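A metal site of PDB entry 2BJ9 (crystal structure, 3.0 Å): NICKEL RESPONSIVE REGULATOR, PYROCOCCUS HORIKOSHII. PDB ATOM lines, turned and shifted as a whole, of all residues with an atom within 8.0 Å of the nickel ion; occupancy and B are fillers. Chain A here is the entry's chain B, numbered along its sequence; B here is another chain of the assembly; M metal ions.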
ATOM      1  N   ASN A  63      -3.348  -6.581  -3.899  1.00  0.00           N
ATOM      2  CA  ASN A  63      -3.646  -5.567  -4.887  1.00  0.00           C
ATOM      3  C   ASN A  63      -4.039  -6.362  -6.116  1.00  0.00           C
ATOM      4  O   ASN A  63      -3.252  -7.181  -6.595  1.00  0.00           O
ATOM      5  CB  ASN A  63      -2.396  -4.728  -5.185  1.00  0.00           C
ATOM      6  CG  ASN A  63      -2.635  -3.657  -6.231  1.00  0.00           C
ATOM      7  OD1 ASN A  63      -2.949  -3.949  -7.386  1.00  0.00           O
ATOM      8  ND2 ASN A  63      -2.494  -2.404  -5.816  1.00  0.00           N
ATOM      9  N   HIS A  64      -5.243  -6.167  -6.636  1.00  0.00           N
ATOM     10  CA  HIS A  64      -5.664  -6.953  -7.792  1.00  0.00           C
ATOM     11  C   HIS A  64      -4.964  -6.570  -9.080  1.00  0.00           C
ATOM     12  O   HIS A  64      -4.772  -7.417  -9.956  1.00  0.00           O
ATOM     13  CB  HIS A  64      -7.182  -6.865  -7.994  1.00  0.00           C
ATOM     14  CG  HIS A  64      -7.670  -5.505  -8.385  1.00  0.00           C
ATOM     15  ND1 HIS A  64      -7.784  -4.473  -7.487  1.00  0.00           N
ATOM     16  CD2 HIS A  64      -8.092  -5.023  -9.570  1.00  0.00           C
ATOM     17  CE1 HIS A  64      -8.254  -3.400  -8.102  1.00  0.00           C
ATOM     18  NE2 HIS A  64      -8.450  -3.708  -9.376  1.00  0.00           N
ATOM     19  N   ASP A  65      -4.565  -5.302  -9.191  1.00  0.00           N
ATOM     20  CA  ASP A  65      -3.891  -4.821 -10.398  1.00  0.00           C
ATOM     21  C   ASP A  65      -2.420  -5.200 -10.456  1.00  0.00           C
ATOM     22  O   ASP A  65      -1.698  -4.765 -11.350  1.00  0.00           O
ATOM     23  CB  ASP A  65      -4.038  -3.309 -10.541  1.00  0.00           C
ATOM     24  CG  ASP A  65      -5.471  -2.889 -10.828  1.00  0.00           C
ATOM     25  OD1 ASP A  65      -6.059  -3.396 -11.823  1.00  0.00           O
ATOM     26  OD2 ASP A  65      -6.004  -2.065 -10.074  1.00  0.00           O
ATOM     27  N   GLU A  66      -1.984  -5.997  -9.481  1.00  0.00           N
ATOM     28  CA  GLU A  66      -0.592  -6.432  -9.434  1.00  0.00           C
ATOM     29  C   GLU A  66      -0.514  -7.818 -10.055  1.00  0.00           C
ATOM     30  O   GLU A  66      -1.506  -8.532 -10.113  1.00  0.00           O
ATOM     31  CB  GLU A  66      -0.111  -6.480  -7.986  1.00  0.00           C
ATOM     32  CG  GLU A  66       1.367  -6.793  -7.820  1.00  0.00           C
ATOM     33  CD  GLU A  66       1.811  -6.764  -6.374  1.00  0.00           C
ATOM     34  OE1 GLU A  66       1.383  -7.642  -5.601  1.00  0.00           O
ATOM     35  OE2 GLU A  66       2.575  -5.850  -6.001  1.00  0.00           O
ATOM     36  N   ASP A  93      -9.800  -0.142  -1.214  1.00  0.00           N
ATOM     37  CA  ASP A  93      -9.631   1.126  -1.886  1.00  0.00           C
ATOM     38  C   ASP A  93      -9.549   0.887  -3.378  1.00  0.00           C
ATOM     39  O   ASP A  93     -10.042  -0.114  -3.885  1.00  0.00           O
ATOM     40  CB  ASP A  93      -8.361   1.830  -1.388  1.00  0.00           C
ATOM     41  CG  ASP A  93      -7.122   0.958  -1.527  1.00  0.00           C
ATOM     42  OD1 ASP A  93      -6.766   0.590  -2.671  1.00  0.00           O
ATOM     43  OD2 ASP A  93      -6.493   0.657  -0.500  1.00  0.00           O
ATOM     44  N   GLU A  94      -8.935   1.826  -4.083  1.00  0.00           N
ATOM     45  CA  GLU A  94      -8.819   1.716  -5.530  1.00  0.00           C
ATOM     46  C   GLU A  94      -7.969   0.529  -5.989  1.00  0.00           C
ATOM     47  O   GLU A  94      -8.160   0.032  -7.094  1.00  0.00           O
ATOM     48  CB  GLU A  94      -8.225   3.027  -6.073  1.00  0.00           C
ATOM     49  CG  GLU A  94      -8.042   3.060  -7.582  1.00  0.00           C
ATOM     50  CD  GLU A  94      -7.244   4.263  -8.029  1.00  0.00           C
ATOM     51  OE1 GLU A  94      -6.960   4.371  -9.248  1.00  0.00           O
ATOM     52  OE2 GLU A  94      -6.899   5.104  -7.174  1.00  0.00           O
ATOM     53  N   HIS A  95      -7.063   0.060  -5.148  1.00  0.00           N
ATOM     54  CA  HIS A  95      -6.187  -1.044  -5.536  1.00  0.00           C
ATOM     55  C   HIS A  95      -6.179  -2.293  -4.688  1.00  0.00           C
ATOM     56  O   HIS A  95      -6.017  -3.403  -5.210  1.00  0.00           O
ATOM     57  CB  HIS A  95      -4.751  -0.529  -5.632  1.00  0.00           C
ATOM     58  CG  HIS A  95      -4.530   0.465  -6.735  1.00  0.00           C
ATOM     59  ND1 HIS A  95      -4.491   0.101  -8.061  1.00  0.00           N
ATOM     60  CD2 HIS A  95      -4.393   1.805  -6.699  1.00  0.00           C
ATOM     61  CE1 HIS A  95      -4.326   1.182  -8.807  1.00  0.00           C
ATOM     62  NE2 HIS A  95      -4.266   2.226  -8.009  1.00  0.00           N
ATOM     63  N   ASN A  96      -6.358  -2.143  -3.372  1.00  0.00           N
ATOM     64  CA  ASN A  96      -6.323  -3.301  -2.494  1.00  0.00           C
ATOM     65  C   ASN A  96      -7.665  -3.916  -2.148  1.00  0.00           C
ATOM     66  O   ASN A  96      -8.648  -3.222  -1.922  1.00  0.00           O
ATOM     67  CB  ASN A  96      -5.606  -2.941  -1.186  1.00  0.00           C
ATOM     68  CG  ASN A  96      -4.193  -2.458  -1.427  1.00  0.00           C
ATOM     69  OD1 ASN A  96      -3.402  -3.117  -2.102  1.00  0.00           O
ATOM     70  ND2 ASN A  96      -3.863  -1.309  -0.860  1.00  0.00           N
ATOM     71  N   CYS A  97      -7.677  -5.243  -2.123  1.00  0.00           N
ATOM     72  CA  CYS A  97      -8.875  -6.005  -1.789  1.00  0.00           C
ATOM     73  C   CYS A  97      -8.574  -6.842  -0.564  1.00  0.00           C
ATOM     74  O   CYS A  97      -7.436  -7.273  -0.356  1.00  0.00           O
ATOM     75  CB  CYS A  97      -9.243  -6.960  -2.936  1.00  0.00           C
ATOM     76  SG  CYS A  97      -9.329  -6.272  -4.604  1.00  0.00           S
ATOM     77  N   LYS B  71     -10.957  -9.597 -14.222  1.00  0.00           N
ATOM     78  CA  LYS B  71     -10.402  -8.271 -13.967  1.00  0.00           C
ATOM     79  C   LYS B  71     -11.398  -7.159 -14.313  1.00  0.00           C
ATOM     80  O   LYS B  71     -11.531  -6.185 -13.574  1.00  0.00           O
ATOM     81  CB  LYS B  71      -9.101  -8.080 -14.750  1.00  0.00           C
ATOM     82  CG  LYS B  71      -8.251  -6.914 -14.255  1.00  0.00           C
ATOM     83  CD  LYS B  71      -6.824  -6.981 -14.795  1.00  0.00           C
ATOM     84  CE  LYS B  71      -6.044  -5.714 -14.466  1.00  0.00           C
ATOM     85  NZ  LYS B  71      -6.584  -4.510 -15.162  1.00  0.00           N
ATOM     86  N   ALA B  72     -12.113  -7.303 -15.425  1.00  0.00           N
ATOM     87  CA  ALA B  72     -13.111  -6.296 -15.796  1.00  0.00           C
ATOM     88  C   ALA B  72     -14.079  -6.094 -14.648  1.00  0.00           C
ATOM     89  O   ALA B  72     -14.527  -4.969 -14.393  1.00  0.00           O
ATOM     90  CB  ALA B  72     -13.879  -6.750 -17.034  1.00  0.00           C
ATOM     91  N   LEU B  73     -14.409  -7.171 -13.950  1.00  0.00           N
ATOM     92  CA  LEU B  73     -15.343  -7.120 -12.827  1.00  0.00           C
ATOM     93  C   LEU B  73     -14.721  -6.401 -11.640  1.00  0.00           C
ATOM     94  O   LEU B  73     -15.383  -5.601 -10.976  1.00  0.00           O
ATOM     95  CB  LEU B  73     -15.758  -8.531 -12.398  1.00  0.00           C
ATOM     96  CG  LEU B  73     -16.827  -9.258 -13.215  1.00  0.00           C
ATOM     97  CD1 LEU B  73     -16.914 -10.701 -12.792  1.00  0.00           C
ATOM     98  CD2 LEU B  73     -18.162  -8.587 -13.007  1.00  0.00           C
ATOM     99  N   LEU B  74     -13.456  -6.698 -11.365  1.00  0.00           N
ATOM    100  CA  LEU B  74     -12.789  -6.056 -10.242  1.00  0.00           C
ATOM    101  C   LEU B  74     -12.557  -4.580 -10.527  1.00  0.00           C
ATOM    102  O   LEU B  74     -12.932  -3.725  -9.713  1.00  0.00           O
ATOM    103  CB  LEU B  74     -11.467  -6.746  -9.957  1.00  0.00           C
ATOM    104  CG  LEU B  74     -11.668  -8.132  -9.325  1.00  0.00           C
ATOM    105  CD1 LEU B  74     -10.319  -8.777  -9.051  1.00  0.00           C
ATOM    106  CD2 LEU B  74     -12.455  -7.974  -8.036  1.00  0.00           C
ATOM    107  N   ASP B  75     -11.961  -4.277 -11.673  1.00  0.00           N
ATOM    108  CA  ASP B  75     -11.718  -2.885 -12.023  1.00  0.00           C
ATOM    109  C   ASP B  75     -13.018  -2.089 -11.976  1.00  0.00           C
ATOM    110  O   ASP B  75     -13.079  -0.998 -11.415  1.00  0.00           O
ATOM    111  CB  ASP B  75     -11.067  -2.779 -13.405  1.00  0.00           C
ATOM    112  CG  ASP B  75      -9.602  -3.207 -13.413  1.00  0.00           C
ATOM    113  OD1 ASP B  75      -8.968  -3.144 -14.497  1.00  0.00           O
ATOM    114  OD2 ASP B  75      -9.062  -3.614 -12.363  1.00  0.00           O
ATOM    115  N   LEU B  76     -14.063  -2.657 -12.559  1.00  0.00           N
ATOM    116  CA  LEU B  76     -15.369  -2.006 -12.590  1.00  0.00           C
ATOM    117  C   LEU B  76     -15.979  -1.813 -11.206  1.00  0.00           C
ATOM    118  O   LEU B  76     -16.695  -0.845 -10.967  1.00  0.00           O
ATOM    119  CB  LEU B  76     -16.335  -2.799 -13.471  1.00  0.00           C
ATOM    120  CG  LEU B  76     -17.771  -2.282 -13.470  1.00  0.00           C
ATOM    121  CD1 LEU B  76     -17.786  -0.908 -14.101  1.00  0.00           C
ATOM    122  CD2 LEU B  76     -18.680  -3.216 -14.232  1.00  0.00           C
ATOM    123  N   GLN B  77     -15.722  -2.752 -10.290  1.00  0.00           N
ATOM    124  CA  GLN B  77     -16.281  -2.647  -8.943  1.00  0.00           C
ATOM    125  C   GLN B  77     -15.534  -1.642  -8.099  1.00  0.00           C
ATOM    126  O   GLN B  77     -16.133  -0.976  -7.262  1.00  0.00           O
ATOM    127  CB  GLN B  77     -16.273  -4.009  -8.241  1.00  0.00           C
ATOM    128  CG  GLN B  77     -17.390  -4.929  -8.676  1.00  0.00           C
ATOM    129  CD  GLN B  77     -17.346  -6.268  -7.991  1.00  0.00           C
ATOM    130  OE1 GLN B  77     -17.436  -6.369  -6.771  1.00  0.00           O
ATOM    131  NE2 GLN B  77     -17.207  -7.324  -8.782  1.00  0.00           N
ATOM    132  N   HIS B  78     -14.222  -1.545  -8.307  1.00  0.00           N
ATOM    133  CA  HIS B  78     -13.400  -0.611  -7.558  1.00  0.00           C
ATOM    134  C   HIS B  78     -13.647   0.824  -7.967  1.00  0.00           C
ATOM    135  O   HIS B  78     -13.154   1.754  -7.318  1.00  0.00           O
ATOM    136  CB  HIS B  78     -11.928  -0.959  -7.716  1.00  0.00           C
ATOM    137  CG  HIS B  78     -11.485  -2.118  -6.864  1.00  0.00           C
ATOM    138  ND1 HIS B  78     -11.351  -2.019  -5.501  1.00  0.00           N
ATOM    139  CD2 HIS B  78     -11.198  -3.394  -7.185  1.00  0.00           C
ATOM    140  CE1 HIS B  78     -10.986  -3.189  -5.017  1.00  0.00           C
ATOM    141  NE2 HIS B  78     -10.884  -4.042  -6.014  1.00  0.00           N
ATOM    142  N   GLU B  79     -14.406   1.016  -9.046  1.00  0.00           N
ATOM    143  CA  GLU B  79     -14.735   2.354  -9.502  1.00  0.00           C
ATOM    144  C   GLU B  79     -15.804   2.883  -8.568  1.00  0.00           C
ATOM    145  O   GLU B  79     -15.908   4.085  -8.351  1.00  0.00           O
ATOM    146  CB  GLU B  79     -15.292   2.331 -10.925  1.00  0.00           C
ATOM    147  CG  GLU B  79     -14.379   1.694 -11.958  1.00  0.00           C
ATOM    148  CD  GLU B  79     -14.782   2.079 -13.379  1.00  0.00           C
ATOM    149  OE1 GLU B  79     -14.179   1.525 -14.330  1.00  0.00           O
ATOM    150  OE2 GLU B  79     -15.686   2.926 -13.546  1.00  0.00           O
HETATM  151 NI    NI M   1      -8.230  -2.043 -10.815  1.00  0.00          NI
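The side-chain carboxylate of Asp 65 lies within salt-bridge range of the side-chain amino group of Lys 71 of chain B, at 3.6 Å.
ND1 of His 64 sits close to SG of Cys 97 (3.7 Å).
ND1 of His 64 is in hydrogen-bond range of O of His 95 (3.1 Å).
The side-chain amide oxygen (OD1) of Asn 63 is in hydrogen-bond range of the backbone NH (N) of Asp 65 (2.8 Å).
A ring nitrogen (ND1) of His 64 sits close to a ring nitrogen (NE2) of His 78 of chain B (3.5 Å).
The side-chain carboxylate (OD2) of Asp 65 lies close to a ring nitrogen (ND1) of His 95, 3.3 Å away.
The side-chain carboxylate (OD1) of Asp 75 of chain B lies within salt-bridge range of the side-chain amino group (NZ) of Lys 71 of chain B, at 2.8 Å.
The nickel ion is bound by NE2 of His 64 (2.2 Å), OD2 of Asp 65 (2.3 Å) and OD2 of Asp 75 of chain B (2.4 Å).
Slightly farther from the nickel ion lies the side-chain carboxylate (OD1) of Asp 65 (2.7 Å).
Along chain A the residues within 4 Å of the nickel ion span positions 64 to 65.
The nearest printed residue that does not touch the nickel ion is Glu 94 (4.3 Å).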
